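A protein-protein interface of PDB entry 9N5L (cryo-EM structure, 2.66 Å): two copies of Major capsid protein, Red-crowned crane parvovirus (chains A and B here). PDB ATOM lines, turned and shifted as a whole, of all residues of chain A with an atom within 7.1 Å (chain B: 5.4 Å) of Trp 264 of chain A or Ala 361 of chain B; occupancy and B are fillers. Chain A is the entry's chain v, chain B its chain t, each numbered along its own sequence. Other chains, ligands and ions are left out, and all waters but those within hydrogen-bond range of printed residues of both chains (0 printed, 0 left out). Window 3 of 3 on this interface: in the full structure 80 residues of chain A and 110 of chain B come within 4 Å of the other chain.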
ATOM      1  N   ASP A 262      13.845  16.361  13.595  1.00  0.00           N
ATOM      2  CA  ASP A 262      12.581  17.040  13.806  1.00  0.00           C
ATOM      3  C   ASP A 262      12.872  18.366  14.482  1.00  0.00           C
ATOM      4  O   ASP A 262      13.973  18.574  14.999  1.00  0.00           O
ATOM      5  CB  ASP A 262      11.640  16.187  14.655  1.00  0.00           C
ATOM      6  CG  ASP A 262      10.234  16.717  14.668  1.00  0.00           C
ATOM      7  OD1 ASP A 262       9.973  17.716  13.973  1.00  0.00           O
ATOM      8  OD2 ASP A 262       9.378  16.130  15.353  1.00  0.00           O
ATOM      9  N   THR A 263      11.912  19.274  14.446  1.00  0.00           N
ATOM     10  CA  THR A 263      12.080  20.527  15.152  1.00  0.00           C
ATOM     11  C   THR A 263      11.000  20.700  16.207  1.00  0.00           C
ATOM     12  O   THR A 263       9.903  20.146  16.103  1.00  0.00           O
ATOM     13  CB  THR A 263      12.059  21.698  14.176  1.00  0.00           C
ATOM     14  OG1 THR A 263      12.369  22.904  14.879  1.00  0.00           O
ATOM     15  CG2 THR A 263      10.704  21.826  13.518  1.00  0.00           C
ATOM     16  N   TRP A 264      11.315  21.488  17.218  1.00  0.00           N
ATOM     17  CA  TRP A 264      10.348  21.817  18.247  1.00  0.00           C
ATOM     18  C   TRP A 264       9.302  22.770  17.687  1.00  0.00           C
ATOM     19  O   TRP A 264       8.195  22.867  18.196  1.00  0.00           O
ATOM     20  CB  TRP A 264      11.039  22.339  19.492  1.00  0.00           C
ATOM     21  CG  TRP A 264      11.706  21.221  20.184  1.00  0.00           C
ATOM     22  CD1 TRP A 264      13.033  20.944  20.201  1.00  0.00           C
ATOM     23  CD2 TRP A 264      11.066  20.173  20.908  1.00  0.00           C
ATOM     24  NE1 TRP A 264      13.267  19.802  20.918  1.00  0.00           N
ATOM     25  CE2 TRP A 264      12.071  19.308  21.365  1.00  0.00           C
ATOM     26  CE3 TRP A 264       9.738  19.890  21.228  1.00  0.00           C
ATOM     27  CZ2 TRP A 264      11.794  18.181  22.123  1.00  0.00           C
ATOM     28  CZ3 TRP A 264       9.466  18.774  21.980  1.00  0.00           C
ATOM     29  CH2 TRP A 264      10.487  17.932  22.420  1.00  0.00           C
ATOM     30  N   GLN A 265       9.686  23.484  16.636  1.00  0.00           N
ATOM     31  CA  GLN A 265       8.817  24.440  15.968  1.00  0.00           C
ATOM     32  C   GLN A 265       7.624  23.781  15.293  1.00  0.00           C
ATOM     33  O   GLN A 265       7.719  22.670  14.797  1.00  0.00           O
ATOM     34  CB  GLN A 265       9.609  25.214  14.919  1.00  0.00           C
ATOM     35  CG  GLN A 265      10.965  25.701  15.386  1.00  0.00           C
ATOM     36  CD  GLN A 265      10.868  26.873  16.332  1.00  0.00           C
ATOM     37  OE1 GLN A 265      11.877  27.412  16.771  1.00  0.00           O
ATOM     38  NE2 GLN A 265       9.649  27.279  16.645  1.00  0.00           N
ATOM     39  N   VAL A 266       6.492  24.470  15.315  1.00  0.00           N
ATOM     40  CA  VAL A 266       5.258  24.012  14.682  1.00  0.00           C
ATOM     41  C   VAL A 266       5.267  24.338  13.191  1.00  0.00           C
ATOM     42  O   VAL A 266       6.149  25.049  12.723  1.00  0.00           O
ATOM     43  CB  VAL A 266       4.031  24.647  15.337  1.00  0.00           C
ATOM     44  CG1 VAL A 266       3.921  24.195  16.781  1.00  0.00           C
ATOM     45  CG2 VAL A 266       4.110  26.160  15.242  1.00  0.00           C
ATOM     46  N   ASP A 267       4.319  23.793  12.433  1.00  0.00           N
ATOM     47  CA  ASP A 267       4.266  24.082  11.010  1.00  0.00           C
ATOM     48  C   ASP A 267       3.635  25.459  10.812  1.00  0.00           C
ATOM     49  O   ASP A 267       3.348  26.182  11.767  1.00  0.00           O
ATOM     50  CB  ASP A 267       3.522  22.987  10.251  1.00  0.00           C
ATOM     51  CG  ASP A 267       2.042  22.948  10.559  1.00  0.00           C
ATOM     52  OD1 ASP A 267       1.587  23.660  11.470  1.00  0.00           O
ATOM     53  OD2 ASP A 267       1.319  22.210   9.866  1.00  0.00           O
ATOM     54  N   ASN A 271       0.694  23.155  13.498  1.00  0.00           N
ATOM     55  CA  ASN A 271       0.683  21.753  13.860  1.00  0.00           C
ATOM     56  C   ASN A 271       2.095  21.183  13.853  1.00  0.00           C
ATOM     57  O   ASN A 271       3.085  21.898  13.694  1.00  0.00           O
ATOM     58  CB  ASN A 271      -0.221  20.994  12.907  1.00  0.00           C
ATOM     59  CG  ASN A 271      -1.644  21.455  13.000  1.00  0.00           C
ATOM     60  OD1 ASN A 271      -2.065  21.985  14.024  1.00  0.00           O
ATOM     61  ND2 ASN A 271      -2.394  21.288  11.924  1.00  0.00           N
ATOM     62  N   ALA A 273       5.481  19.717  12.843  1.00  0.00           N
ATOM     63  CA  ALA A 273       6.260  19.918  11.641  1.00  0.00           C
ATOM     64  C   ALA A 273       6.833  18.573  11.263  1.00  0.00           C
ATOM     65  O   ALA A 273       7.682  18.029  11.960  1.00  0.00           O
ATOM     66  CB  ALA A 273       7.373  20.916  11.900  1.00  0.00           C
ATOM     67  N   CYS B 171      15.953  25.635  17.034  1.00  0.00           N
ATOM     68  CA  CYS B 171      15.256  24.704  17.909  1.00  0.00           C
ATOM     69  C   CYS B 171      14.839  23.440  17.171  1.00  0.00           C
ATOM     70  O   CYS B 171      13.658  23.173  16.952  1.00  0.00           O
ATOM     71  CB  CYS B 171      14.058  25.385  18.563  1.00  0.00           C
ATOM     72  SG  CYS B 171      14.530  26.758  19.629  1.00  0.00           S
ATOM     73  N   GLN B 172      15.835  22.660  16.772  1.00  0.00           N
ATOM     74  CA  GLN B 172      15.589  21.293  16.363  1.00  0.00           C
ATOM     75  C   GLN B 172      15.936  20.341  17.496  1.00  0.00           C
ATOM     76  O   GLN B 172      16.446  20.735  18.547  1.00  0.00           O
ATOM     77  CB  GLN B 172      16.384  20.957  15.110  1.00  0.00           C
ATOM     78  CG  GLN B 172      15.758  21.448  13.841  1.00  0.00           C
ATOM     79  CD  GLN B 172      16.578  21.110  12.634  1.00  0.00           C
ATOM     80  OE1 GLN B 172      17.796  21.199  12.656  1.00  0.00           O
ATOM     81  NE2 GLN B 172      15.921  20.617  11.607  1.00  0.00           N
ATOM     82  N   THR B 173      15.686  19.056  17.263  1.00  0.00           N
ATOM     83  CA  THR B 173      15.989  18.057  18.275  1.00  0.00           C
ATOM     84  C   THR B 173      17.485  17.877  18.444  1.00  0.00           C
ATOM     85  O   THR B 173      17.922  17.115  19.310  1.00  0.00           O
ATOM     86  CB  THR B 173      15.315  16.746  17.913  1.00  0.00           C
ATOM     87  OG1 THR B 173      15.767  16.318  16.628  1.00  0.00           O
ATOM     88  CG2 THR B 173      13.831  16.952  17.859  1.00  0.00           C
ATOM     89  N   PHE B 338       5.294  26.887  19.333  1.00  0.00           N
ATOM     90  CA  PHE B 338       6.285  25.836  19.233  1.00  0.00           C
ATOM     91  C   PHE B 338       5.984  24.775  20.272  1.00  0.00           C
ATOM     92  O   PHE B 338       5.263  25.020  21.238  1.00  0.00           O
ATOM     93  CB  PHE B 338       7.700  26.377  19.419  1.00  0.00           C
ATOM     94  CG  PHE B 338       7.882  27.159  20.673  1.00  0.00           C
ATOM     95  CD1 PHE B 338       8.209  26.535  21.857  1.00  0.00           C
ATOM     96  CD2 PHE B 338       7.735  28.525  20.667  1.00  0.00           C
ATOM     97  CE1 PHE B 338       8.378  27.262  23.003  1.00  0.00           C
ATOM     98  CE2 PHE B 338       7.904  29.252  21.811  1.00  0.00           C
ATOM     99  CZ  PHE B 338       8.228  28.620  22.977  1.00  0.00           C
ATOM    100  N   TRP B 339       6.542  23.596  20.058  1.00  0.00           N
ATOM    101  CA  TRP B 339       6.421  22.527  21.030  1.00  0.00           C
ATOM    102  C   TRP B 339       7.496  22.637  22.091  1.00  0.00           C
ATOM    103  O   TRP B 339       8.636  23.008  21.811  1.00  0.00           O
ATOM    104  CB  TRP B 339       6.512  21.165  20.356  1.00  0.00           C
ATOM    105  CG  TRP B 339       5.322  20.807  19.585  1.00  0.00           C
ATOM    106  CD1 TRP B 339       4.207  21.555  19.410  1.00  0.00           C
ATOM    107  CD2 TRP B 339       5.088  19.571  18.924  1.00  0.00           C
ATOM    108  NE1 TRP B 339       3.298  20.872  18.651  1.00  0.00           N
ATOM    109  CE2 TRP B 339       3.817  19.646  18.342  1.00  0.00           C
ATOM    110  CE3 TRP B 339       5.841  18.409  18.755  1.00  0.00           C
ATOM    111  CZ2 TRP B 339       3.281  18.606  17.608  1.00  0.00           C
ATOM    112  CZ3 TRP B 339       5.308  17.383  18.031  1.00  0.00           C
ATOM    113  CH2 TRP B 339       4.040  17.483  17.467  1.00  0.00           C
ATOM    114  N   THR B 340       7.120  22.319  23.320  1.00  0.00           N
ATOM    115  CA  THR B 340       8.074  22.130  24.390  1.00  0.00           C
ATOM    116  C   THR B 340       7.902  20.725  24.937  1.00  0.00           C
ATOM    117  O   THR B 340       6.784  20.202  24.961  1.00  0.00           O
ATOM    118  CB  THR B 340       7.880  23.150  25.515  1.00  0.00           C
ATOM    119  OG1 THR B 340       6.533  23.087  25.986  1.00  0.00           O
ATOM    120  CG2 THR B 340       8.173  24.538  25.030  1.00  0.00           C
ATOM    121  N   PRO B 341       8.983  20.084  25.359  1.00  0.00           N
ATOM    122  CA  PRO B 341       8.854  18.760  25.968  1.00  0.00           C
ATOM    123  C   PRO B 341       7.999  18.835  27.216  1.00  0.00           C
ATOM    124  O   PRO B 341       8.132  19.756  28.022  1.00  0.00           O
ATOM    125  CB  PRO B 341      10.298  18.392  26.311  1.00  0.00           C
ATOM    126  CG  PRO B 341      11.125  19.239  25.443  1.00  0.00           C
ATOM    127  CD  PRO B 341      10.384  20.509  25.258  1.00  0.00           C
ATOM    128  N   LYS B 342       7.102  17.864  27.376  1.00  0.00           N
ATOM    129  CA  LYS B 342       6.398  17.758  28.646  1.00  0.00           C
ATOM    130  C   LYS B 342       7.374  17.475  29.774  1.00  0.00           C
ATOM    131  O   LYS B 342       7.451  18.230  30.749  1.00  0.00           O
ATOM    132  CB  LYS B 342       5.326  16.679  28.580  1.00  0.00           C
ATOM    133  CG  LYS B 342       4.180  17.030  27.680  1.00  0.00           C
ATOM    134  CD  LYS B 342       3.141  15.946  27.694  1.00  0.00           C
ATOM    135  CE  LYS B 342       1.957  16.319  26.840  1.00  0.00           C
ATOM    136  NZ  LYS B 342       0.953  15.230  26.812  1.00  0.00           N
ATOM    137  N   ILE B 356       9.443  14.136  17.016  1.00  0.00           N
ATOM    138  CA  ILE B 356       9.076  14.304  18.406  1.00  0.00           C
ATOM    139  C   ILE B 356       7.681  13.736  18.550  1.00  0.00           C
ATOM    140  O   ILE B 356       6.809  14.031  17.739  1.00  0.00           O
ATOM    141  CB  ILE B 356       9.030  15.788  18.795  1.00  0.00           C
ATOM    142  CG1 ILE B 356      10.397  16.434  18.598  1.00  0.00           C
ATOM    143  CG2 ILE B 356       8.557  15.945  20.229  1.00  0.00           C
ATOM    144  CD1 ILE B 356      10.343  17.935  18.460  1.00  0.00           C
ATOM    145  N   ASN B 357       7.462  12.931  19.579  1.00  0.00           N
ATOM    146  CA  ASN B 357       6.146  12.359  19.794  1.00  0.00           C
ATOM    147  C   ASN B 357       5.214  13.482  20.207  1.00  0.00           C
ATOM    148  O   ASN B 357       5.569  14.320  21.028  1.00  0.00           O
ATOM    149  CB  ASN B 357       6.196  11.280  20.868  1.00  0.00           C
ATOM    150  CG  ASN B 357       4.936  10.447  20.911  1.00  0.00           C
ATOM    151  OD1 ASN B 357       4.107  10.513  20.007  1.00  0.00           O
ATOM    152  ND2 ASN B 357       4.785   9.657  21.963  1.00  0.00           N
ATOM    153  N   THR B 358       4.013  13.493  19.650  1.00  0.00           N
ATOM    154  CA  THR B 358       3.053  14.537  19.968  1.00  0.00           C
ATOM    155  C   THR B 358       2.640  14.516  21.431  1.00  0.00           C
ATOM    156  O   THR B 358       2.482  15.562  22.054  1.00  0.00           O
ATOM    157  CB  THR B 358       1.795  14.422  19.095  1.00  0.00           C
ATOM    158  OG1 THR B 358       1.148  13.172  19.356  1.00  0.00           O
ATOM    159  CG2 THR B 358       2.163  14.500  17.627  1.00  0.00           C
ATOM    160  N   SER B 359       2.460  13.321  21.978  1.00  0.00           N
ATOM    161  CA  SER B 359       2.028  13.178  23.360  1.00  0.00           C
ATOM    162  C   SER B 359       3.161  13.487  24.325  1.00  0.00           C
ATOM    163  O   SER B 359       2.949  13.567  25.538  1.00  0.00           O
ATOM    164  CB  SER B 359       1.493  11.769  23.589  1.00  0.00           C
ATOM    165  OG  SER B 359       2.510  10.811  23.376  1.00  0.00           O
ATOM    166  N   THR B 360       4.377  13.645  23.807  1.00  0.00           N
ATOM    167  CA  THR B 360       5.506  13.944  24.676  1.00  0.00           C
ATOM    168  C   THR B 360       5.798  15.435  24.710  1.00  0.00           C
ATOM    169  O   THR B 360       6.755  15.871  25.356  1.00  0.00           O
ATOM    170  CB  THR B 360       6.739  13.172  24.219  1.00  0.00           C
ATOM    171  OG1 THR B 360       7.056  13.533  22.872  1.00  0.00           O
ATOM    172  CG2 THR B 360       6.480  11.683  24.288  1.00  0.00           C
ATOM    173  N   ALA B 361       4.996  16.231  24.019  1.00  0.00           N
ATOM    174  CA  ALA B 361       5.265  17.653  23.864  1.00  0.00           C
ATOM    175  C   ALA B 361       4.037  18.475  24.215  1.00  0.00           C
ATOM    176  O   ALA B 361       2.903  18.031  24.015  1.00  0.00           O
ATOM    177  CB  ALA B 361       5.709  17.974  22.437  1.00  0.00           C
ATOM    178  N   TYR B 362       4.275  19.664  24.751  1.00  0.00           N
ATOM    179  CA  TYR B 362       3.237  20.669  24.873  1.00  0.00           C
ATOM    180  C   TYR B 362       3.275  21.603  23.677  1.00  0.00           C
ATOM    181  O   TYR B 362       4.341  21.998  23.211  1.00  0.00           O
ATOM    182  CB  TYR B 362       3.432  21.485  26.146  1.00  0.00           C
ATOM    183  CG  TYR B 362       3.184  20.736  27.421  1.00  0.00           C
ATOM    184  CD1 TYR B 362       2.039  19.979  27.591  1.00  0.00           C
ATOM    185  CD2 TYR B 362       4.106  20.772  28.449  1.00  0.00           C
ATOM    186  CE1 TYR B 362       1.810  19.300  28.757  1.00  0.00           C
ATOM    187  CE2 TYR B 362       3.889  20.089  29.613  1.00  0.00           C
ATOM    188  CZ  TYR B 362       2.742  19.356  29.764  1.00  0.00           C
ATOM    189  OH  TYR B 362       2.528  18.671  30.934  1.00  0.00           O
ATOM    190  N   LYS B 363       2.101  21.977  23.193  1.00  0.00           N
ATOM    191  CA  LYS B 363       1.988  23.020  22.188  1.00  0.00           C
ATOM    192  C   LYS B 363       1.876  24.346  22.920  1.00  0.00           C
ATOM    193  O   LYS B 363       0.878  24.603  23.598  1.00  0.00           O
ATOM    194  CB  LYS B 363       0.780  22.805  21.285  1.00  0.00           C
ATOM    195  CG  LYS B 363       0.618  23.894  20.253  1.00  0.00           C
ATOM    196  CD  LYS B 363      -0.606  23.682  19.401  1.00  0.00           C
ATOM    197  CE  LYS B 363      -0.796  24.838  18.444  1.00  0.00           C
ATOM    198  NZ  LYS B 363      -1.997  24.664  17.592  1.00  0.00           N
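Of the 8 printed residues of chain A, 5 touch a printed residue of chain B.
Hydrophobic or aromatic side chains of chain A within 4 Å of the printed part of chain B: Trp 264 and Val 266.
Of the 16 printed residues of chain B, 9 touch a printed residue of chain A.
Printed residues of chain B that touch a printed residue of chain A: Cys 171, Gln 172, Thr 173, Phe 338, Trp 339, Thr 340, Pro 341, Ile 356 and Ala 361.
Hydrophobic or aromatic side chains of chain B within 4 Å of the printed part of chain A: Phe 338, Trp 339, Pro 341, Ile 356 and Ala 361.
Among the printed residues, 18 pairs touch across the chains.
Among the printed residues, no Asp or Glu carboxylate lies within 4 Å of a Lys or Arg side-chain nitrogen of the other chain.
N of Gln 265 of chain A lies close to OG1 of Thr 263 of chain A.
The backbone NH (N) of Tyr 362 of chain B is in hydrogen-bond range of the backbone carbonyl oxygen (O) of Thr 340 of chain B (2.6 Å).
Asp 262 of chain A touches Gln 172 of chain B (O to CB, 3.4 Å).
Thr 263 of chain A touches Ile 356 of chain B (O to CD1, 3.3 Å).
Phe 338 of chain B touches Trp 264 of chain A (C to O, 3.6 Å).
Trp 264 of chain A touches Thr 340 of chain B (CZ3 to C, 3.9 Å).
Ile 356 of chain B touches Trp 264 of chain A (CD1 to CD2, 3.4 Å).
Trp 264 of chain A touches Ala 361 of chain B (CZ3 to CB, 3.9 Å).
Gln 265 of chain A touches Cys 171 of chain B.
CB of Phe 338 of chain B touches NE2 of Gln 265 of chain A (3.5 Å).
CG1 of Val 266 of chain A touches CA of Phe 338 of chain B (3.8 Å).
Val 266 of chain A touches Trp 339 of chain B.
Trp 264 of chain A touches just these residues of chain B: Cys 171, Gln 172, Phe 338, Trp 339, Thr 340, Pro 341, Ile 356 and Ala 361.
Printed residues of chain A within 4 Å of Ala 361 of chain B: Trp 264 (3.9 Å).
Of the printed residues of chain A, Gln 172 of chain B touches Asp 262 (3.4 Å), Thr 263 (3.7 Å) and Trp 264 (3.8 Å).
Of the printed residues of chain A, Phe 338 of chain B touches Trp 264 (3.6 Å), Gln 265 (3.5 Å) and Val 266 (3.8 Å).
Printed residues of chain B within 4 Å of Gln 265 of chain A: Cys 171 and Phe 338.
Of the printed residues of chain B, Val 266 of chain A touches Phe 338 and Trp 339.
Printed residues of chain A within 4 Å of Cys 171 of chain B: Thr 263, Trp 264 and Gln 265.
Lys 363 of chain B touches none of the printed residues of chain A.
The nearest printed residue of chain B that does not touch Val 266 of chain A is Lys 363 of chain B (4.8 Å).
No position is printed for both chains.
Of the 18 pairs that touch across the chains among the printed residues, none has its exchanged pair printed and touching as well.
N of Trp 264 of chain A sits at hydrogen-bond distance from O of Cys 171 of chain B (2.9 Å).
O of Cys 171 of chain B is in hydrogen-bond range of OG1 of Thr 263 of chain A (2.5 Å).
N of Ile 356 of chain B lies close to OD2 of Asp 262 of chain A (2.6 Å).
O of Asp 262 of chain A sits at hydrogen-bond distance from N of Thr 173 of chain B, at 2.9 Å.
N of Trp 339 of chain B sits at hydrogen-bond distance from O of Trp 264 of chain A (2.6 Å).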
